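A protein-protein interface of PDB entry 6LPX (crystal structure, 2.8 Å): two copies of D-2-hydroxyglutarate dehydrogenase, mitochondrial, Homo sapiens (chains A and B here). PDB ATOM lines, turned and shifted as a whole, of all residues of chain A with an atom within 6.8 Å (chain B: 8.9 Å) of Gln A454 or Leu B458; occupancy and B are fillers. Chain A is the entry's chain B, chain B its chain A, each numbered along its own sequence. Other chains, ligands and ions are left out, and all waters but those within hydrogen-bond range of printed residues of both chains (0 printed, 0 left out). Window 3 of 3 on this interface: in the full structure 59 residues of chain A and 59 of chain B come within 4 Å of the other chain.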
ATOM      1  N   GLY A 447     -28.744  24.438  28.579  1.00  0.00           N
ATOM      2  CA  GLY A 447     -29.080  23.046  28.861  1.00  0.00           C
ATOM      3  C   GLY A 447     -29.322  22.223  27.609  1.00  0.00           C
ATOM      4  O   GLY A 447     -28.895  21.063  27.521  1.00  0.00           O
ATOM      5  N   ALA A 448     -29.956  22.827  26.597  1.00  0.00           N
ATOM      6  CA  ALA A 448     -30.120  22.140  25.321  1.00  0.00           C
ATOM      7  C   ALA A 448     -28.775  21.837  24.662  1.00  0.00           C
ATOM      8  O   ALA A 448     -28.532  20.709  24.205  1.00  0.00           O
ATOM      9  CB  ALA A 448     -30.973  23.005  24.393  1.00  0.00           C
ATOM     10  N   LEU A 449     -27.880  22.827  24.615  1.00  0.00           N
ATOM     11  CA  LEU A 449     -26.568  22.596  24.027  1.00  0.00           C
ATOM     12  C   LEU A 449     -25.821  21.489  24.763  1.00  0.00           C
ATOM     13  O   LEU A 449     -25.122  20.668  24.144  1.00  0.00           O
ATOM     14  CB  LEU A 449     -25.769  23.890  24.026  1.00  0.00           C
ATOM     15  CG  LEU A 449     -26.325  25.051  23.193  1.00  0.00           C
ATOM     16  CD1 LEU A 449     -25.445  26.282  23.372  1.00  0.00           C
ATOM     17  CD2 LEU A 449     -26.502  24.707  21.719  1.00  0.00           C
ATOM     18  N   GLN A 450     -26.007  21.410  26.083  1.00  0.00           N
ATOM     19  CA  GLN A 450     -25.343  20.356  26.840  1.00  0.00           C
ATOM     20  C   GLN A 450     -25.913  18.990  26.476  1.00  0.00           C
ATOM     21  O   GLN A 450     -25.159  18.025  26.298  1.00  0.00           O
ATOM     22  CB  GLN A 450     -25.461  20.629  28.342  1.00  0.00           C
ATOM     23  CG  GLN A 450     -24.669  19.657  29.218  1.00  0.00           C
ATOM     24  CD  GLN A 450     -25.028  19.734  30.699  1.00  0.00           C
ATOM     25  OE1 GLN A 450     -25.568  20.736  31.175  1.00  0.00           O
ATOM     26  NE2 GLN A 450     -24.714  18.671  31.438  1.00  0.00           N
ATOM     27  N   LEU A 451     -27.239  18.884  26.389  1.00  0.00           N
ATOM     28  CA  LEU A 451     -27.840  17.614  25.993  1.00  0.00           C
ATOM     29  C   LEU A 451     -27.376  17.187  24.599  1.00  0.00           C
ATOM     30  O   LEU A 451     -27.154  15.995  24.347  1.00  0.00           O
ATOM     31  CB  LEU A 451     -29.362  17.706  26.045  1.00  0.00           C
ATOM     32  CG  LEU A 451     -30.099  16.448  25.584  1.00  0.00           C
ATOM     33  CD1 LEU A 451     -29.669  15.235  26.388  1.00  0.00           C
ATOM     34  CD2 LEU A 451     -31.600  16.640  25.681  1.00  0.00           C
ATOM     35  N   MET A 452     -27.194  18.154  23.691  1.00  0.00           N
ATOM     36  CA  MET A 452     -26.642  17.838  22.373  1.00  0.00           C
ATOM     37  C   MET A 452     -25.245  17.250  22.485  1.00  0.00           C
ATOM     38  O   MET A 452     -24.901  16.284  21.788  1.00  0.00           O
ATOM     39  CB  MET A 452     -26.613  19.112  21.527  1.00  0.00           C
ATOM     40  CG  MET A 452     -27.995  19.580  21.190  1.00  0.00           C
ATOM     41  SD  MET A 452     -28.198  21.171  20.393  1.00  0.00           S
ATOM     42  CE  MET A 452     -26.620  21.467  19.610  1.00  0.00           C
ATOM     43  N   GLN A 453     -24.429  17.814  23.364  1.00  0.00           N
ATOM     44  CA  GLN A 453     -23.087  17.276  23.557  1.00  0.00           C
ATOM     45  C   GLN A 453     -23.133  15.861  24.125  1.00  0.00           C
ATOM     46  O   GLN A 453     -22.346  14.992  23.735  1.00  0.00           O
ATOM     47  CB  GLN A 453     -22.254  18.236  24.397  1.00  0.00           C
ATOM     48  CG  GLN A 453     -22.143  19.578  23.684  1.00  0.00           C
ATOM     49  CD  GLN A 453     -21.457  20.652  24.492  1.00  0.00           C
ATOM     50  OE1 GLN A 453     -21.394  20.574  25.721  1.00  0.00           O
ATOM     51  NE2 GLN A 453     -20.925  21.664  23.802  1.00  0.00           N
ATOM     52  N   GLN A 454     -24.067  15.607  25.033  1.00  0.00           N
ATOM     53  CA  GLN A 454     -24.210  14.263  25.582  1.00  0.00           C
ATOM     54  C   GLN A 454     -24.633  13.264  24.509  1.00  0.00           C
ATOM     55  O   GLN A 454     -24.151  12.124  24.483  1.00  0.00           O
ATOM     56  CB  GLN A 454     -25.256  14.314  26.689  1.00  0.00           C
ATOM     57  CG  GLN A 454     -24.843  15.130  27.875  1.00  0.00           C
ATOM     58  CD  GLN A 454     -25.991  15.352  28.832  1.00  0.00           C
ATOM     59  OE1 GLN A 454     -26.620  16.420  28.819  1.00  0.00           O
ATOM     60  NE2 GLN A 454     -26.311  14.340  29.621  1.00  0.00           N
ATOM     61  N   LEU A 455     -25.517  13.681  23.605  1.00  0.00           N
ATOM     62  CA  LEU A 455     -25.893  12.823  22.485  1.00  0.00           C
ATOM     63  C   LEU A 455     -24.679  12.494  21.621  1.00  0.00           C
ATOM     64  O   LEU A 455     -24.462  11.332  21.253  1.00  0.00           O
ATOM     65  CB  LEU A 455     -26.980  13.501  21.656  1.00  0.00           C
ATOM     66  CG  LEU A 455     -28.331  13.544  22.356  1.00  0.00           C
ATOM     67  CD1 LEU A 455     -29.364  14.238  21.483  1.00  0.00           C
ATOM     68  CD2 LEU A 455     -28.785  12.148  22.773  1.00  0.00           C
ATOM     69  N   LYS A 456     -23.863  13.511  21.325  1.00  0.00           N
ATOM     70  CA  LYS A 456     -22.639  13.313  20.548  1.00  0.00           C
ATOM     71  C   LYS A 456     -21.715  12.316  21.233  1.00  0.00           C
ATOM     72  O   LYS A 456     -21.166  11.416  20.588  1.00  0.00           O
ATOM     73  CB  LYS A 456     -21.933  14.660  20.362  1.00  0.00           C
ATOM     74  CG  LYS A 456     -20.572  14.632  19.674  1.00  0.00           C
ATOM     75  CD  LYS A 456     -20.580  14.130  18.240  1.00  0.00           C
ATOM     76  CE  LYS A 456     -19.146  14.104  17.702  1.00  0.00           C
ATOM     77  NZ  LYS A 456     -19.030  13.792  16.253  1.00  0.00           N
ATOM     78  N   ALA A 457     -21.527  12.476  22.546  1.00  0.00           N
ATOM     79  CA  ALA A 457     -20.671  11.575  23.318  1.00  0.00           C
ATOM     80  C   ALA A 457     -21.183  10.145  23.299  1.00  0.00           C
ATOM     81  O   ALA A 457     -20.387   9.200  23.267  1.00  0.00           O
ATOM     82  CB  ALA A 457     -20.580  12.047  24.767  1.00  0.00           C
ATOM     83  N   LEU A 458     -22.501   9.964  23.393  1.00  0.00           N
ATOM     84  CA  LEU A 458     -23.074   8.625  23.296  1.00  0.00           C
ATOM     85  C   LEU A 458     -22.814   7.999  21.937  1.00  0.00           C
ATOM     86  O   LEU A 458     -22.345   6.857  21.841  1.00  0.00           O
ATOM     87  CB  LEU A 458     -24.576   8.679  23.578  1.00  0.00           C
ATOM     88  CG  LEU A 458     -25.391   7.390  23.443  1.00  0.00           C
ATOM     89  CD1 LEU A 458     -25.031   6.362  24.505  1.00  0.00           C
ATOM     90  CD2 LEU A 458     -26.868   7.740  23.529  1.00  0.00           C
ATOM     91  N   LEU A 459     -23.065   8.748  20.876  1.00  0.00           N
ATOM     92  CA  LEU A 459     -23.043   8.167  19.543  1.00  0.00           C
ATOM     93  C   LEU A 459     -21.661   8.165  18.904  1.00  0.00           C
ATOM     94  O   LEU A 459     -21.392   7.328  18.031  1.00  0.00           O
ATOM     95  CB  LEU A 459     -24.064   8.888  18.659  1.00  0.00           C
ATOM     96  CG  LEU A 459     -25.492   8.438  18.977  1.00  0.00           C
ATOM     97  CD1 LEU A 459     -26.528   9.389  18.429  1.00  0.00           C
ATOM     98  CD2 LEU A 459     -25.699   7.061  18.388  1.00  0.00           C
ATOM     99  N   LEU A 471     -21.429  21.594  17.069  1.00  0.00           N
ATOM    100  CA  LEU A 471     -21.697  21.911  18.463  1.00  0.00           C
ATOM    101  C   LEU A 471     -20.702  22.957  18.946  1.00  0.00           C
ATOM    102  O   LEU A 471     -19.645  23.144  18.336  1.00  0.00           O
ATOM    103  CB  LEU A 471     -21.564  20.654  19.327  1.00  0.00           C
ATOM    104  CG  LEU A 471     -22.326  19.413  18.870  1.00  0.00           C
ATOM    105  CD1 LEU A 471     -21.921  18.220  19.711  1.00  0.00           C
ATOM    106  CD2 LEU A 471     -23.815  19.641  18.970  1.00  0.00           C
ATOM    107  N   HIS B  74     -35.944  11.643  42.065  1.00  0.00           N
ATOM    108  CA  HIS B  74     -34.621  11.172  41.661  1.00  0.00           C
ATOM    109  C   HIS B  74     -33.745  10.902  42.867  1.00  0.00           C
ATOM    110  O   HIS B  74     -33.078   9.860  42.941  1.00  0.00           O
ATOM    111  CB  HIS B  74     -33.937  12.197  40.752  1.00  0.00           C
ATOM    112  CG  HIS B  74     -32.608  11.742  40.214  1.00  0.00           C
ATOM    113  ND1 HIS B  74     -31.410  12.249  40.680  1.00  0.00           N
ATOM    114  CD2 HIS B  74     -32.284  10.786  39.312  1.00  0.00           C
ATOM    115  CE1 HIS B  74     -30.409  11.662  40.051  1.00  0.00           C
ATOM    116  NE2 HIS B  74     -30.912  10.764  39.220  1.00  0.00           N
ATOM    117  N   LEU B 184     -36.860  16.666  32.858  1.00  0.00           N
ATOM    118  CA  LEU B 184     -36.150  15.395  32.858  1.00  0.00           C
ATOM    119  C   LEU B 184     -36.212  14.711  34.225  1.00  0.00           C
ATOM    120  O   LEU B 184     -36.623  15.297  35.234  1.00  0.00           O
ATOM    121  CB  LEU B 184     -34.702  15.606  32.436  1.00  0.00           C
ATOM    122  CG  LEU B 184     -34.523  16.306  31.088  1.00  0.00           C
ATOM    123  CD1 LEU B 184     -33.043  16.513  30.782  1.00  0.00           C
ATOM    124  CD2 LEU B 184     -35.189  15.457  29.998  1.00  0.00           C
ATOM    125  N   ALA B 185     -35.798  13.435  34.233  1.00  0.00           N
ATOM    126  CA  ALA B 185     -35.950  12.588  35.415  1.00  0.00           C
ATOM    127  C   ALA B 185     -35.290  13.185  36.654  1.00  0.00           C
ATOM    128  O   ALA B 185     -35.807  13.036  37.765  1.00  0.00           O
ATOM    129  CB  ALA B 185     -35.391  11.190  35.134  1.00  0.00           C
ATOM    130  N   ASP B 186     -34.161  13.874  36.501  1.00  0.00           N
ATOM    131  CA  ASP B 186     -33.524  14.445  37.679  1.00  0.00           C
ATOM    132  C   ASP B 186     -34.081  15.813  38.047  1.00  0.00           C
ATOM    133  O   ASP B 186     -33.577  16.435  38.981  1.00  0.00           O
ATOM    134  CB  ASP B 186     -32.010  14.525  37.494  1.00  0.00           C
ATOM    135  CG  ASP B 186     -31.592  15.517  36.420  1.00  0.00           C
ATOM    136  OD1 ASP B 186     -32.478  16.144  35.786  1.00  0.00           O
ATOM    137  OD2 ASP B 186     -30.358  15.668  36.218  1.00  0.00           O
ATOM    138  N   THR B 188     -34.112  18.400  35.840  1.00  0.00           N
ATOM    139  CA  THR B 188     -33.591  19.392  34.904  1.00  0.00           C
ATOM    140  C   THR B 188     -34.673  19.835  33.933  1.00  0.00           C
ATOM    141  O   THR B 188     -35.408  19.007  33.389  1.00  0.00           O
ATOM    142  CB  THR B 188     -32.397  18.834  34.129  1.00  0.00           C
ATOM    143  OG1 THR B 188     -31.407  18.372  35.050  1.00  0.00           O
ATOM    144  CG2 THR B 188     -31.802  19.894  33.219  1.00  0.00           C
ATOM    145  N   LEU B 190     -35.519  21.201  30.478  1.00  0.00           N
ATOM    146  CA  LEU B 190     -35.010  21.318  29.125  1.00  0.00           C
ATOM    147  C   LEU B 190     -35.936  22.250  28.366  1.00  0.00           C
ATOM    148  O   LEU B 190     -37.137  21.967  28.228  1.00  0.00           O
ATOM    149  CB  LEU B 190     -34.928  19.953  28.446  1.00  0.00           C
ATOM    150  CG  LEU B 190     -34.511  19.971  26.982  1.00  0.00           C
ATOM    151  CD1 LEU B 190     -33.104  20.501  26.877  1.00  0.00           C
ATOM    152  CD2 LEU B 190     -34.615  18.567  26.400  1.00  0.00           C
ATOM    153  N   TYR B 203     -29.189  20.087  17.023  1.00  0.00           N
ATOM    154  CA  TYR B 203     -30.026  18.903  16.928  1.00  0.00           C
ATOM    155  C   TYR B 203     -31.453  19.248  17.325  1.00  0.00           C
ATOM    156  O   TYR B 203     -31.689  20.083  18.203  1.00  0.00           O
ATOM    157  CB  TYR B 203     -29.516  17.776  17.828  1.00  0.00           C
ATOM    158  CG  TYR B 203     -28.074  17.361  17.650  1.00  0.00           C
ATOM    159  CD1 TYR B 203     -27.424  17.532  16.436  1.00  0.00           C
ATOM    160  CD2 TYR B 203     -27.374  16.743  18.689  1.00  0.00           C
ATOM    161  CE1 TYR B 203     -26.114  17.130  16.274  1.00  0.00           C
ATOM    162  CE2 TYR B 203     -26.059  16.348  18.534  1.00  0.00           C
ATOM    163  CZ  TYR B 203     -25.435  16.542  17.322  1.00  0.00           C
ATOM    164  OH  TYR B 203     -24.129  16.147  17.134  1.00  0.00           O
ATOM    165  N   LEU B 205     -33.733  18.373  19.293  1.00  0.00           N
ATOM    166  CA  LEU B 205     -33.872  17.572  20.509  1.00  0.00           C
ATOM    167  C   LEU B 205     -35.326  17.263  20.850  1.00  0.00           C
ATOM    168  O   LEU B 205     -35.625  16.156  21.318  1.00  0.00           O
ATOM    169  CB  LEU B 205     -33.242  18.306  21.689  1.00  0.00           C
ATOM    170  CG  LEU B 205     -31.736  18.528  21.682  1.00  0.00           C
ATOM    171  CD1 LEU B 205     -31.413  19.533  22.760  1.00  0.00           C
ATOM    172  CD2 LEU B 205     -30.956  17.245  21.876  1.00  0.00           C
ATOM    173  N   LEU B 208     -36.929  13.801  20.124  1.00  0.00           N
ATOM    174  CA  LEU B 208     -36.791  12.645  21.004  1.00  0.00           C
ATOM    175  C   LEU B 208     -38.000  12.464  21.904  1.00  0.00           C
ATOM    176  O   LEU B 208     -38.321  11.341  22.298  1.00  0.00           O
ATOM    177  CB  LEU B 208     -35.555  12.790  21.877  1.00  0.00           C
ATOM    178  CG  LEU B 208     -34.195  12.626  21.235  1.00  0.00           C
ATOM    179  CD1 LEU B 208     -33.142  12.859  22.298  1.00  0.00           C
ATOM    180  CD2 LEU B 208     -34.090  11.215  20.706  1.00  0.00           C
ATOM    181  N   THR B 215     -41.123   8.190  29.042  1.00  0.00           N
ATOM    182  CA  THR B 215     -39.980   7.445  29.541  1.00  0.00           C
ATOM    183  C   THR B 215     -38.699   8.254  29.484  1.00  0.00           C
ATOM    184  O   THR B 215     -37.689   7.825  30.047  1.00  0.00           O
ATOM    185  CB  THR B 215     -39.771   6.194  28.719  1.00  0.00           C
ATOM    186  OG1 THR B 215     -39.494   6.587  27.369  1.00  0.00           O
ATOM    187  CG2 THR B 215     -41.046   5.365  28.746  1.00  0.00           C
ATOM    188  N   LEU B 216     -38.704   9.385  28.774  1.00  0.00           N
ATOM    189  CA  LEU B 216     -37.514  10.201  28.638  1.00  0.00           C
ATOM    190  C   LEU B 216     -37.641  11.560  29.302  1.00  0.00           C
ATOM    191  O   LEU B 216     -36.626  12.246  29.466  1.00  0.00           O
ATOM    192  CB  LEU B 216     -37.170  10.386  27.152  1.00  0.00           C
ATOM    193  CG  LEU B 216     -36.900   9.105  26.346  1.00  0.00           C
ATOM    194  CD1 LEU B 216     -36.544   9.411  24.885  1.00  0.00           C
ATOM    195  CD2 LEU B 216     -35.821   8.237  26.995  1.00  0.00           C
ATOM    196  N   LEU B 451     -30.261   0.940  20.677  1.00  0.00           N
ATOM    197  CA  LEU B 451     -30.020   2.376  20.769  1.00  0.00           C
ATOM    198  C   LEU B 451     -31.119   3.065  21.581  1.00  0.00           C
ATOM    199  O   LEU B 451     -30.850   4.009  22.337  1.00  0.00           O
ATOM    200  CB  LEU B 451     -29.935   2.979  19.370  1.00  0.00           C
ATOM    201  CG  LEU B 451     -29.760   4.491  19.297  1.00  0.00           C
ATOM    202  CD1 LEU B 451     -28.507   4.916  20.085  1.00  0.00           C
ATOM    203  CD2 LEU B 451     -29.700   4.942  17.853  1.00  0.00           C
ATOM    204  N   MET B 452     -32.368   2.623  21.424  1.00  0.00           N
ATOM    205  CA  MET B 452     -33.448   3.152  22.252  1.00  0.00           C
ATOM    206  C   MET B 452     -33.139   2.984  23.734  1.00  0.00           C
ATOM    207  O   MET B 452     -33.306   3.915  24.530  1.00  0.00           O
ATOM    208  CB  MET B 452     -34.761   2.460  21.909  1.00  0.00           C
ATOM    209  CG  MET B 452     -35.249   2.711  20.503  1.00  0.00           C
ATOM    210  SD  MET B 452     -36.854   1.941  20.235  1.00  0.00           S
ATOM    211  CE  MET B 452     -36.972   2.036  18.445  1.00  0.00           C
ATOM    212  N   GLN B 453     -32.694   1.787  24.121  1.00  0.00           N
ATOM    213  CA  GLN B 453     -32.324   1.544  25.516  1.00  0.00           C
ATOM    214  C   GLN B 453     -31.148   2.414  25.957  1.00  0.00           C
ATOM    215  O   GLN B 453     -31.116   2.892  27.097  1.00  0.00           O
ATOM    216  CB  GLN B 453     -32.011   0.060  25.731  1.00  0.00           C
ATOM    217  CG  GLN B 453     -31.566  -0.287  27.149  1.00  0.00           C
ATOM    218  CD  GLN B 453     -32.615   0.061  28.217  1.00  0.00           C
ATOM    219  OE1 GLN B 453     -33.819  -0.170  28.031  1.00  0.00           O
ATOM    220  NE2 GLN B 453     -32.155   0.618  29.347  1.00  0.00           N
ATOM    221  N   GLN B 454     -30.182   2.655  25.066  1.00  0.00           N
ATOM    222  CA  GLN B 454     -29.070   3.533  25.424  1.00  0.00           C
ATOM    223  C   GLN B 454     -29.546   4.958  25.674  1.00  0.00           C
ATOM    224  O   GLN B 454     -29.060   5.632  26.592  1.00  0.00           O
ATOM    225  CB  GLN B 454     -28.012   3.520  24.330  1.00  0.00           C
ATOM    226  CG  GLN B 454     -27.322   2.200  24.122  1.00  0.00           C
ATOM    227  CD  GLN B 454     -26.358   2.265  22.959  1.00  0.00           C
ATOM    228  OE1 GLN B 454     -26.644   1.778  21.858  1.00  0.00           O
ATOM    229  NE2 GLN B 454     -25.203   2.878  23.195  1.00  0.00           N
ATOM    230  N   LEU B 455     -30.491   5.443  24.865  1.00  0.00           N
ATOM    231  CA  LEU B 455     -31.028   6.773  25.127  1.00  0.00           C
ATOM    232  C   LEU B 455     -31.799   6.814  26.438  1.00  0.00           C
ATOM    233  O   LEU B 455     -31.695   7.792  27.196  1.00  0.00           O
ATOM    234  CB  LEU B 455     -31.906   7.255  23.975  1.00  0.00           C
ATOM    235  CG  LEU B 455     -31.158   7.601  22.692  1.00  0.00           C
ATOM    236  CD1 LEU B 455     -32.112   7.713  21.533  1.00  0.00           C
ATOM    237  CD2 LEU B 455     -30.399   8.893  22.886  1.00  0.00           C
ATOM    238  N   LYS B 456     -32.607   5.784  26.704  1.00  0.00           N
ATOM    239  CA  LYS B 456     -33.288   5.714  27.995  1.00  0.00           C
ATOM    240  C   LYS B 456     -32.290   5.773  29.149  1.00  0.00           C
ATOM    241  O   LYS B 456     -32.514   6.480  30.138  1.00  0.00           O
ATOM    242  CB  LYS B 456     -34.140   4.445  28.072  1.00  0.00           C
ATOM    243  CG  LYS B 456     -34.781   4.149  29.434  1.00  0.00           C
ATOM    244  CD  LYS B 456     -35.684   5.280  29.939  1.00  0.00           C
ATOM    245  CE  LYS B 456     -36.257   4.937  31.330  1.00  0.00           C
ATOM    246  NZ  LYS B 456     -37.386   5.784  31.829  1.00  0.00           N
ATOM    247  N   ALA B 457     -31.191   5.022  29.042  1.00  0.00           N
ATOM    248  CA  ALA B 457     -30.176   5.011  30.090  1.00  0.00           C
ATOM    249  C   ALA B 457     -29.460   6.345  30.229  1.00  0.00           C
ATOM    250  O   ALA B 457     -29.125   6.757  31.345  1.00  0.00           O
ATOM    251  CB  ALA B 457     -29.157   3.920  29.798  1.00  0.00           C
ATOM    252  N   LEU B 458     -29.244   7.046  29.118  1.00  0.00           N
ATOM    253  CA  LEU B 458     -28.622   8.362  29.190  1.00  0.00           C
ATOM    254  C   LEU B 458     -29.542   9.378  29.857  1.00  0.00           C
ATOM    255  O   LEU B 458     -29.125  10.098  30.772  1.00  0.00           O
ATOM    256  CB  LEU B 458     -28.201   8.817  27.789  1.00  0.00           C
ATOM    257  CG  LEU B 458     -27.731  10.267  27.649  1.00  0.00           C
ATOM    258  CD1 LEU B 458     -26.575  10.563  28.578  1.00  0.00           C
ATOM    259  CD2 LEU B 458     -27.325  10.571  26.222  1.00  0.00           C
ATOM    260  N   LEU B 459     -30.807   9.422  29.451  1.00  0.00           N
ATOM    261  CA  LEU B 459     -31.677  10.480  29.946  1.00  0.00           C
ATOM    262  C   LEU B 459     -32.247  10.188  31.330  1.00  0.00           C
ATOM    263  O   LEU B 459     -32.610  11.129  32.050  1.00  0.00           O
ATOM    264  CB  LEU B 459     -32.804  10.755  28.950  1.00  0.00           C
ATOM    265  CG  LEU B 459     -32.371  11.500  27.689  1.00  0.00           C
ATOM    266  CD1 LEU B 459     -33.437  11.456  26.638  1.00  0.00           C
ATOM    267  CD2 LEU B 459     -32.106  12.931  28.067  1.00  0.00           C
ATOM    268  N   ASP B 460     -32.385   8.912  31.701  1.00  0.00           N
ATOM    269  CA  ASP B 460     -33.000   8.534  32.974  1.00  0.00           C
ATOM    270  C   ASP B 460     -32.302   7.283  33.496  1.00  0.00           C
ATOM    271  O   ASP B 460     -32.872   6.184  33.504  1.00  0.00           O
ATOM    272  CB  ASP B 460     -34.500   8.316  32.786  1.00  0.00           C
ATOM    273  CG  ASP B 460     -35.190   7.822  34.031  1.00  0.00           C
ATOM    274  OD1 ASP B 460     -36.356   7.394  33.896  1.00  0.00           O
ATOM    275  OD2 ASP B 460     -34.593   7.884  35.131  1.00  0.00           O
ATOM    276  N   PRO B 461     -31.052   7.418  33.948  1.00  0.00           N
ATOM    277  CA  PRO B 461     -30.300   6.229  34.392  1.00  0.00           C
ATOM    278  C   PRO B 461     -30.946   5.458  35.535  1.00  0.00           C
ATOM    279  O   PRO B 461     -30.834   4.225  35.568  1.00  0.00           O
ATOM    280  CB  PRO B 461     -28.936   6.809  34.800  1.00  0.00           C
ATOM    281  CG  PRO B 461     -29.163   8.266  34.979  1.00  0.00           C
ATOM    282  CD  PRO B 461     -30.238   8.640  34.009  1.00  0.00           C
ATOM    283  N   LYS B 462     -31.662   6.123  36.444  1.00  0.00           N
ATOM    284  CA  LYS B 462     -32.340   5.380  37.503  1.00  0.00           C
ATOM    285  C   LYS B 462     -33.618   4.708  37.020  1.00  0.00           C
ATOM    286  O   LYS B 462     -34.163   3.866  37.741  1.00  0.00           O
ATOM    287  CB  LYS B 462     -32.657   6.276  38.702  1.00  0.00           C
ATOM    288  CG  LYS B 462     -31.446   6.856  39.411  1.00  0.00           C
ATOM    289  CD  LYS B 462     -31.879   7.449  40.744  1.00  0.00           C
ATOM    290  CE  LYS B 462     -30.740   8.071  41.504  1.00  0.00           C
ATOM    291  NZ  LYS B 462     -31.128   8.333  42.915  1.00  0.00           N
ATOM    292  N   GLY B 463     -34.106   5.068  35.837  1.00  0.00           N
ATOM    293  CA  GLY B 463     -35.315   4.476  35.303  1.00  0.00           C
ATOM    294  C   GLY B 463     -36.580   4.776  36.064  1.00  0.00           C
ATOM    295  O   GLY B 463     -37.513   3.970  36.037  1.00  0.00           O
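Gln A454 touches just one residue of chain B: Leu B458 (3.9 Å). Of chain A, only Gln A454 and Leu A458 come within 4 Å of Leu B458. Of the printed residues of chain A, Tyr B203 touches Met A452 (3.5 Å) and Leu A471 (3.9 Å). Of the printed residues of chain B, Ala A448 touches Leu B190 (3.7 Å) and Leu B205 (3.4 Å). Of the printed residues of chain A, Leu B190 touches Ala A448 (3.7 Å) and Leu A451 (3.6 Å). Of the printed residues of chain B, Leu A471 touches Tyr B203. Thr B188 touches none of the printed residues of chain A. Asp B460 touches none of the printed residues of chain A. The nearest residue of chain B that does not touch Gln A454 is Leu B459 (6.2 Å). The nearest printed residue of chain B that does not touch Ala A448 is Tyr B203 (6.8 Å).
CD1 of Leu B205 touches O of Ala A448, at 3.4 Å. Leu B190 touches Leu A451. Leu A451 touches Leu B459 (CD1 to CD2, 3.8 Å). Met A452 touches Leu B205 (CG to CD1, 3.8 Å). Gln A454 touches Leu B458 (NE2 to CD1, 3.9 Å). Leu B205 touches Leu A455. Gln B454 touches Leu A458. Leu A458 touches Leu B455 (CD2 to CD2, 3.8 Å). Leu B458 touches Leu A458 (CD2 to CD2, 3.9 Å). CD2 of Leu A471 touches CZ of Tyr B203 (3.9 Å).
O of Gln A450 sits close to OE1 of Gln A454, at 3.3 Å.
Along chain B the printed residues that touch a printed residue of chain A span positions 190 to 459. Of the 14 printed residues of chain A, 8 touch a printed residue of chain B. Hydrophobic or aromatic side chains of chain A within 4 Å of the printed part of chain B: Ala A448, Leu A451, Met A452, Leu A455, Leu A458, Leu A459 and Leu A471.
Leu A451 touches Leu B459, and with the chains exchanged Leu A459 touches Leu B451. Gln A454 touches Leu B458, and with the chains exchanged Leu A458 touches Gln B454. Leu B455 touches its own counterpart, Leu A455. Leu B458 touches its own counterpart, Leu A458.
SD of Met A452 sits at hydrogen-bond distance from N of Tyr B203, 3.7 Å away.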
